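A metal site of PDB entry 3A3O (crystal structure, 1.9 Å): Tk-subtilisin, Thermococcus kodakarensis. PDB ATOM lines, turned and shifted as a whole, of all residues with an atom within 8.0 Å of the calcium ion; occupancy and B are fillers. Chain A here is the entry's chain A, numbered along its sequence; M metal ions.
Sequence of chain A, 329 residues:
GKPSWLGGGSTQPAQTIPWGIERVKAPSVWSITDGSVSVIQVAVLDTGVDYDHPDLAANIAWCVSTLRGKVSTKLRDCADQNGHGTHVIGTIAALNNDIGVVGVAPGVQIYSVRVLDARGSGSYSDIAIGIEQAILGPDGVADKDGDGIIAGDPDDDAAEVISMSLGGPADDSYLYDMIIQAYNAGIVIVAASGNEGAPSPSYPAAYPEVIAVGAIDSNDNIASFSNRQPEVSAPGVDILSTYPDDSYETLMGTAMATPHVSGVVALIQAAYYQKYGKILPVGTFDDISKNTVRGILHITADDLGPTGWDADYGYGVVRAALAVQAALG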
ATOM      1  N   GLN A  12       8.222 -19.265  10.884  1.00  0.00           N
ATOM      2  CA  GLN A  12       8.470 -19.469   9.404  1.00  0.00           C
ATOM      3  C   GLN A  12       8.094 -18.220   8.612  1.00  0.00           C
ATOM      4  O   GLN A  12       6.979 -17.724   8.747  1.00  0.00           O
ATOM      5  CB  GLN A  12       7.686 -20.673   8.867  1.00  0.00           C
ATOM      6  CG  GLN A  12       8.236 -22.044   9.274  1.00  0.00           C
ATOM      7  CD  GLN A  12       9.605 -22.343   8.656  1.00  0.00           C
ATOM      8  OE1 GLN A  12       9.874 -21.996   7.507  1.00  0.00           O
ATOM      9  NE2 GLN A  12      10.490 -22.954   9.432  1.00  0.00           N
ATOM     10  N   PRO A  13       9.010 -17.725   7.749  1.00  0.00           N
ATOM     11  CA  PRO A  13       8.669 -16.569   6.920  1.00  0.00           C
ATOM     12  C   PRO A  13       7.677 -16.897   5.809  1.00  0.00           C
ATOM     13  O   PRO A  13       7.581 -18.072   5.397  1.00  0.00           O
ATOM     14  CB  PRO A  13      10.015 -16.155   6.308  1.00  0.00           C
ATOM     15  CG  PRO A  13      10.856 -17.439   6.321  1.00  0.00           C
ATOM     16  CD  PRO A  13      10.375 -18.241   7.516  1.00  0.00           C
ATOM     17  N   ALA A  14       6.954 -15.870   5.321  1.00  0.00           N
ATOM     18  CA  ALA A  14       6.071 -15.979   4.154  1.00  0.00           C
ATOM     19  C   ALA A  14       6.874 -16.361   2.913  1.00  0.00           C
ATOM     20  O   ALA A  14       8.043 -15.949   2.776  1.00  0.00           O
ATOM     21  CB  ALA A  14       5.323 -14.667   3.921  1.00  0.00           C
ATOM     22  N   GLN A  15       6.246 -17.136   2.026  1.00  0.00           N
ATOM     23  CA  GLN A  15       6.932 -17.671   0.833  1.00  0.00           C
ATOM     24  C   GLN A  15       7.383 -16.585  -0.144  1.00  0.00           C
ATOM     25  O   GLN A  15       6.623 -15.660  -0.458  1.00  0.00           O
ATOM     26  CB  GLN A  15       6.051 -18.686   0.094  1.00  0.00           C
ATOM     27  CG  GLN A  15       6.730 -19.364  -1.106  1.00  0.00           C
ATOM     28  CD  GLN A  15       5.959 -20.528  -1.644  1.00  0.00           C
ATOM     29  OE1 GLN A  15       6.008 -21.620  -1.075  1.00  0.00           O
ATOM     30  NE2 GLN A  15       5.221 -20.308  -2.734  1.00  0.00           N
ATOM     31  N   THR A  16       8.643 -16.686  -0.604  1.00  0.00           N
ATOM     32  CA  THR A  16       9.079 -15.948  -1.796  1.00  0.00           C
ATOM     33  C   THR A  16       9.496 -16.914  -2.857  1.00  0.00           C
ATOM     34  O   THR A  16       9.881 -18.042  -2.546  1.00  0.00           O
ATOM     35  CB  THR A  16      10.423 -15.218  -1.637  1.00  0.00           C
ATOM     36  OG1 THR A  16      11.017 -15.481  -0.355  1.00  0.00           O
ATOM     37  CG2 THR A  16      10.333 -13.759  -2.031  1.00  0.00           C
ATOM     38  N   HIS A  53      12.348 -30.453   7.797  1.00  0.00           N
ATOM     39  CA  HIS A  53      12.131 -29.057   7.432  1.00  0.00           C
ATOM     40  C   HIS A  53      10.701 -28.870   6.928  1.00  0.00           C
ATOM     41  O   HIS A  53      10.238 -29.624   6.072  1.00  0.00           O
ATOM     42  CB  HIS A  53      13.150 -28.605   6.381  1.00  0.00           C
ATOM     43  CG  HIS A  53      13.149 -27.126   6.149  1.00  0.00           C
ATOM     44  ND1 HIS A  53      14.269 -26.352   6.319  1.00  0.00           N
ATOM     45  CD2 HIS A  53      12.160 -26.287   5.775  1.00  0.00           C
ATOM     46  CE1 HIS A  53      13.984 -25.093   6.029  1.00  0.00           C
ATOM     47  NE2 HIS A  53      12.702 -25.020   5.716  1.00  0.00           N
ATOM     48  N   PRO A  54       9.945 -27.902   7.482  1.00  0.00           N
ATOM     49  CA  PRO A  54       8.537 -27.724   7.045  1.00  0.00           C
ATOM     50  C   PRO A  54       8.383 -27.415   5.556  1.00  0.00           C
ATOM     51  O   PRO A  54       7.315 -27.660   4.958  1.00  0.00           O
ATOM     52  CB  PRO A  54       8.048 -26.515   7.868  1.00  0.00           C
ATOM     53  CG  PRO A  54       8.947 -26.466   9.059  1.00  0.00           C
ATOM     54  CD  PRO A  54      10.311 -26.971   8.578  1.00  0.00           C
ATOM     55  N   ASP A  55       9.425 -26.874   4.935  1.00  0.00           N
ATOM     56  CA  ASP A  55       9.340 -26.568   3.493  1.00  0.00           C
ATOM     57  C   ASP A  55       9.906 -27.661   2.587  1.00  0.00           C
ATOM     58  O   ASP A  55      10.003 -27.462   1.366  1.00  0.00           O
ATOM     59  CB  ASP A  55       9.962 -25.204   3.145  1.00  0.00           C
ATOM     60  CG  ASP A  55       9.117 -24.444   2.123  1.00  0.00           C
ATOM     61  OD1 ASP A  55       7.897 -24.709   2.011  1.00  0.00           O
ATOM     62  OD2 ASP A  55       9.627 -23.554   1.418  1.00  0.00           O
ATOM     63  N   LEU A  56      10.264 -28.806   3.200  1.00  0.00           N
ATOM     64  CA  LEU A  56      10.826 -29.958   2.478  1.00  0.00           C
ATOM     65  C   LEU A  56      10.151 -31.288   2.767  1.00  0.00           C
ATOM     66  O   LEU A  56      10.126 -32.196   1.911  1.00  0.00           O
ATOM     67  CB  LEU A  56      12.313 -30.120   2.811  1.00  0.00           C
ATOM     68  CG  LEU A  56      13.345 -29.049   2.410  1.00  0.00           C
ATOM     69  CD1 LEU A  56      14.708 -29.594   2.751  1.00  0.00           C
ATOM     70  CD2 LEU A  56      13.273 -28.718   0.932  1.00  0.00           C
ATOM     71  N   ALA A  93      13.118 -28.737  -4.879  1.00  0.00           N
ATOM     72  CA  ALA A  93      11.838 -29.330  -4.422  1.00  0.00           C
ATOM     73  C   ALA A  93      11.198 -28.685  -3.205  1.00  0.00           C
ATOM     74  O   ALA A  93      10.287 -29.294  -2.590  1.00  0.00           O
ATOM     75  CB  ALA A  93      12.037 -30.804  -4.166  1.00  0.00           C
ATOM     76  N   ALA A  94      11.636 -27.464  -2.847  1.00  0.00           N
ATOM     77  CA  ALA A  94      10.934 -26.760  -1.748  1.00  0.00           C
ATOM     78  C   ALA A  94       9.439 -26.632  -2.111  1.00  0.00           C
ATOM     79  O   ALA A  94       9.094 -26.366  -3.263  1.00  0.00           O
ATOM     80  CB  ALA A  94      11.545 -25.398  -1.488  1.00  0.00           C
ATOM     81  N   LEU A  95       8.557 -26.835  -1.132  1.00  0.00           N
ATOM     82  CA  LEU A  95       7.119 -26.928  -1.398  1.00  0.00           C
ATOM     83  C   LEU A  95       6.506 -25.574  -1.760  1.00  0.00           C
ATOM     84  O   LEU A  95       6.926 -24.522  -1.236  1.00  0.00           O
ATOM     85  CB  LEU A  95       6.437 -27.512  -0.149  1.00  0.00           C
ATOM     86  CG  LEU A  95       6.805 -28.968   0.152  1.00  0.00           C
ATOM     87  CD1 LEU A  95       6.764 -29.295   1.673  1.00  0.00           C
ATOM     88  CD2 LEU A  95       5.891 -29.917  -0.619  1.00  0.00           C
ATOM     89  N   ASN A  96       5.523 -25.607  -2.653  1.00  0.00           N
ATOM     90  CA  ASN A  96       4.773 -24.411  -3.025  1.00  0.00           C
ATOM     91  C   ASN A  96       3.609 -24.276  -2.034  1.00  0.00           C
ATOM     92  O   ASN A  96       2.630 -25.015  -2.115  1.00  0.00           O
ATOM     93  CB  ASN A  96       4.246 -24.541  -4.438  1.00  0.00           C
ATOM     94  CG  ASN A  96       3.637 -23.248  -4.963  1.00  0.00           C
ATOM     95  OD1 ASN A  96       3.650 -22.230  -4.271  1.00  0.00           O
ATOM     96  ND2 ASN A  96       3.109 -23.286  -6.174  1.00  0.00           N
ATOM     97  N   ASN A  97       3.751 -23.361  -1.081  1.00  0.00           N
ATOM     98  CA  ASN A  97       2.808 -23.247   0.036  1.00  0.00           C
ATOM     99  C   ASN A  97       2.854 -21.817   0.572  1.00  0.00           C
ATOM    100  O   ASN A  97       3.193 -20.895  -0.163  1.00  0.00           O
ATOM    101  CB  ASN A  97       3.140 -24.312   1.130  1.00  0.00           C
ATOM    102  CG  ASN A  97       4.606 -24.253   1.623  1.00  0.00           C
ATOM    103  OD1 ASN A  97       5.335 -23.287   1.370  1.00  0.00           O
ATOM    104  ND2 ASN A  97       5.026 -25.284   2.371  1.00  0.00           N
ATOM    105  N   ASP A  98       2.598 -21.643   1.862  1.00  0.00           N
ATOM    106  CA  ASP A  98       2.565 -20.306   2.427  1.00  0.00           C
ATOM    107  C   ASP A  98       3.867 -19.833   3.047  1.00  0.00           C
ATOM    108  O   ASP A  98       3.928 -18.724   3.558  1.00  0.00           O
ATOM    109  CB  ASP A  98       1.399 -20.185   3.438  1.00  0.00           C
ATOM    110  CG  ASP A  98       0.049 -20.467   2.802  1.00  0.00           C
ATOM    111  OD1 ASP A  98      -0.243 -19.902   1.709  1.00  0.00           O
ATOM    112  OD2 ASP A  98      -0.741 -21.262   3.382  1.00  0.00           O
ATOM    113  N   ILE A  99       4.906 -20.664   2.995  1.00  0.00           N
ATOM    114  CA  ILE A  99       6.148 -20.400   3.721  1.00  0.00           C
ATOM    115  C   ILE A  99       7.433 -20.553   2.894  1.00  0.00           C
ATOM    116  O   ILE A  99       7.465 -21.290   1.914  1.00  0.00           O
ATOM    117  CB  ILE A  99       6.284 -21.313   4.979  1.00  0.00           C
ATOM    118  CG1 ILE A  99       6.183 -22.805   4.588  1.00  0.00           C
ATOM    119  CG2 ILE A  99       5.190 -20.958   6.040  1.00  0.00           C
ATOM    120  CD1 ILE A  99       6.767 -23.744   5.625  1.00  0.00           C
ATOM    121  N   GLY A 100       8.482 -19.857   3.301  1.00  0.00           N
ATOM    122  CA  GLY A 100       9.835 -20.199   2.899  1.00  0.00           C
ATOM    123  C   GLY A 100      10.135 -19.880   1.456  1.00  0.00           C
ATOM    124  O   GLY A 100      10.076 -18.716   1.048  1.00  0.00           O
ATOM    125  N   VAL A 101      10.507 -20.886   0.673  1.00  0.00           N
ATOM    126  CA  VAL A 101      10.853 -20.657  -0.732  1.00  0.00           C
ATOM    127  C   VAL A 101      10.030 -21.629  -1.584  1.00  0.00           C
ATOM    128  O   VAL A 101       9.024 -22.159  -1.101  1.00  0.00           O
ATOM    129  CB  VAL A 101      12.388 -20.772  -0.959  1.00  0.00           C
ATOM    130  CG1 VAL A 101      13.136 -19.598  -0.296  1.00  0.00           C
ATOM    131  CG2 VAL A 101      12.947 -22.154  -0.458  1.00  0.00           C
ATOM    132  N   VAL A 102      10.411 -21.868  -2.838  1.00  0.00           N
ATOM    133  CA  VAL A 102       9.727 -22.851  -3.674  1.00  0.00           C
ATOM    134  C   VAL A 102      10.760 -23.375  -4.672  1.00  0.00           C
ATOM    135  O   VAL A 102      11.561 -22.600  -5.169  1.00  0.00           O
ATOM    136  CB  VAL A 102       8.468 -22.259  -4.387  1.00  0.00           C
ATOM    137  CG1 VAL A 102       8.817 -21.076  -5.328  1.00  0.00           C
ATOM    138  CG2 VAL A 102       7.657 -23.337  -5.095  1.00  0.00           C
ATOM    139  N   GLY A 103      10.725 -24.687  -4.942  1.00  0.00           N
ATOM    140  CA  GLY A 103      11.711 -25.316  -5.839  1.00  0.00           C
ATOM    141  C   GLY A 103      11.269 -25.187  -7.283  1.00  0.00           C
ATOM    142  O   GLY A 103      10.148 -24.755  -7.577  1.00  0.00           O
ATOM    143  N   PRO A 106       8.307 -28.203  -7.373  1.00  0.00           N
ATOM    144  CA  PRO A 106       7.892 -28.204  -5.991  1.00  0.00           C
ATOM    145  C   PRO A 106       7.033 -29.398  -5.524  1.00  0.00           C
ATOM    146  O   PRO A 106       6.748 -29.468  -4.331  1.00  0.00           O
ATOM    147  CB  PRO A 106       7.161 -26.863  -5.838  1.00  0.00           C
ATOM    148  CG  PRO A 106       6.716 -26.468  -7.153  1.00  0.00           C
ATOM    149  CD  PRO A 106       7.673 -27.122  -8.149  1.00  0.00           C
ATOM    150  N   THR A 242      16.388 -23.468   1.359  1.00  0.00           N
ATOM    151  CA  THR A 242      16.278 -24.071   2.679  1.00  0.00           C
ATOM    152  C   THR A 242      17.677 -24.328   3.296  1.00  0.00           C
ATOM    153  O   THR A 242      18.668 -24.548   2.579  1.00  0.00           O
ATOM    154  CB  THR A 242      15.444 -25.374   2.604  1.00  0.00           C
ATOM    155  OG1 THR A 242      15.895 -26.146   1.478  1.00  0.00           O
ATOM    156  CG2 THR A 242      13.938 -25.019   2.360  1.00  0.00           C
ATOM    157  N   TYR A 248      16.638 -20.842   6.404  1.00  0.00           N
ATOM    158  CA  TYR A 248      16.902 -20.480   4.993  1.00  0.00           C
ATOM    159  C   TYR A 248      18.263 -19.807   4.961  1.00  0.00           C
ATOM    160  O   TYR A 248      18.705 -19.240   5.978  1.00  0.00           O
ATOM    161  CB  TYR A 248      15.763 -19.583   4.397  1.00  0.00           C
ATOM    162  CG  TYR A 248      14.437 -20.248   4.550  1.00  0.00           C
ATOM    163  CD1 TYR A 248      13.714 -20.114   5.750  1.00  0.00           C
ATOM    164  CD2 TYR A 248      13.954 -21.130   3.581  1.00  0.00           C
ATOM    165  CE1 TYR A 248      12.551 -20.794   5.964  1.00  0.00           C
ATOM    166  CE2 TYR A 248      12.776 -21.813   3.775  1.00  0.00           C
ATOM    167  CZ  TYR A 248      12.075 -21.643   4.979  1.00  0.00           C
ATOM    168  OH  TYR A 248      10.909 -22.332   5.191  1.00  0.00           O
HETATM  169 CA    CA M   1       7.427 -22.969   0.335  1.00  0.00          CA
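Six residues have an atom within 4 Å of the calcium ion: Gln 15, Asp 55, Leu 95, Asn 97, Ile 99 and Val 101.
Along chain A the residues within 4 Å of the calcium ion span positions 15 to 101.
NE2 of Gln 15 is in hydrogen-bond range of OD1 of Asn 96, 2.9 Å away.
N of Gln 15 lies within hydrogen-bond range of O of Asp 98 (3.2 Å).
The calcium ion is bound by O of Leu 95 (2.3 Å), O of Val 101 (2.3 Å), O of Ile 99 (2.3 Å), OD1 of Asn 97 (2.4 Å), OE1 of Gln 15 (2.4 Å), OD1 of Asp 55 (2.5 Å) and OD2 of Asp 55 (2.5 Å).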
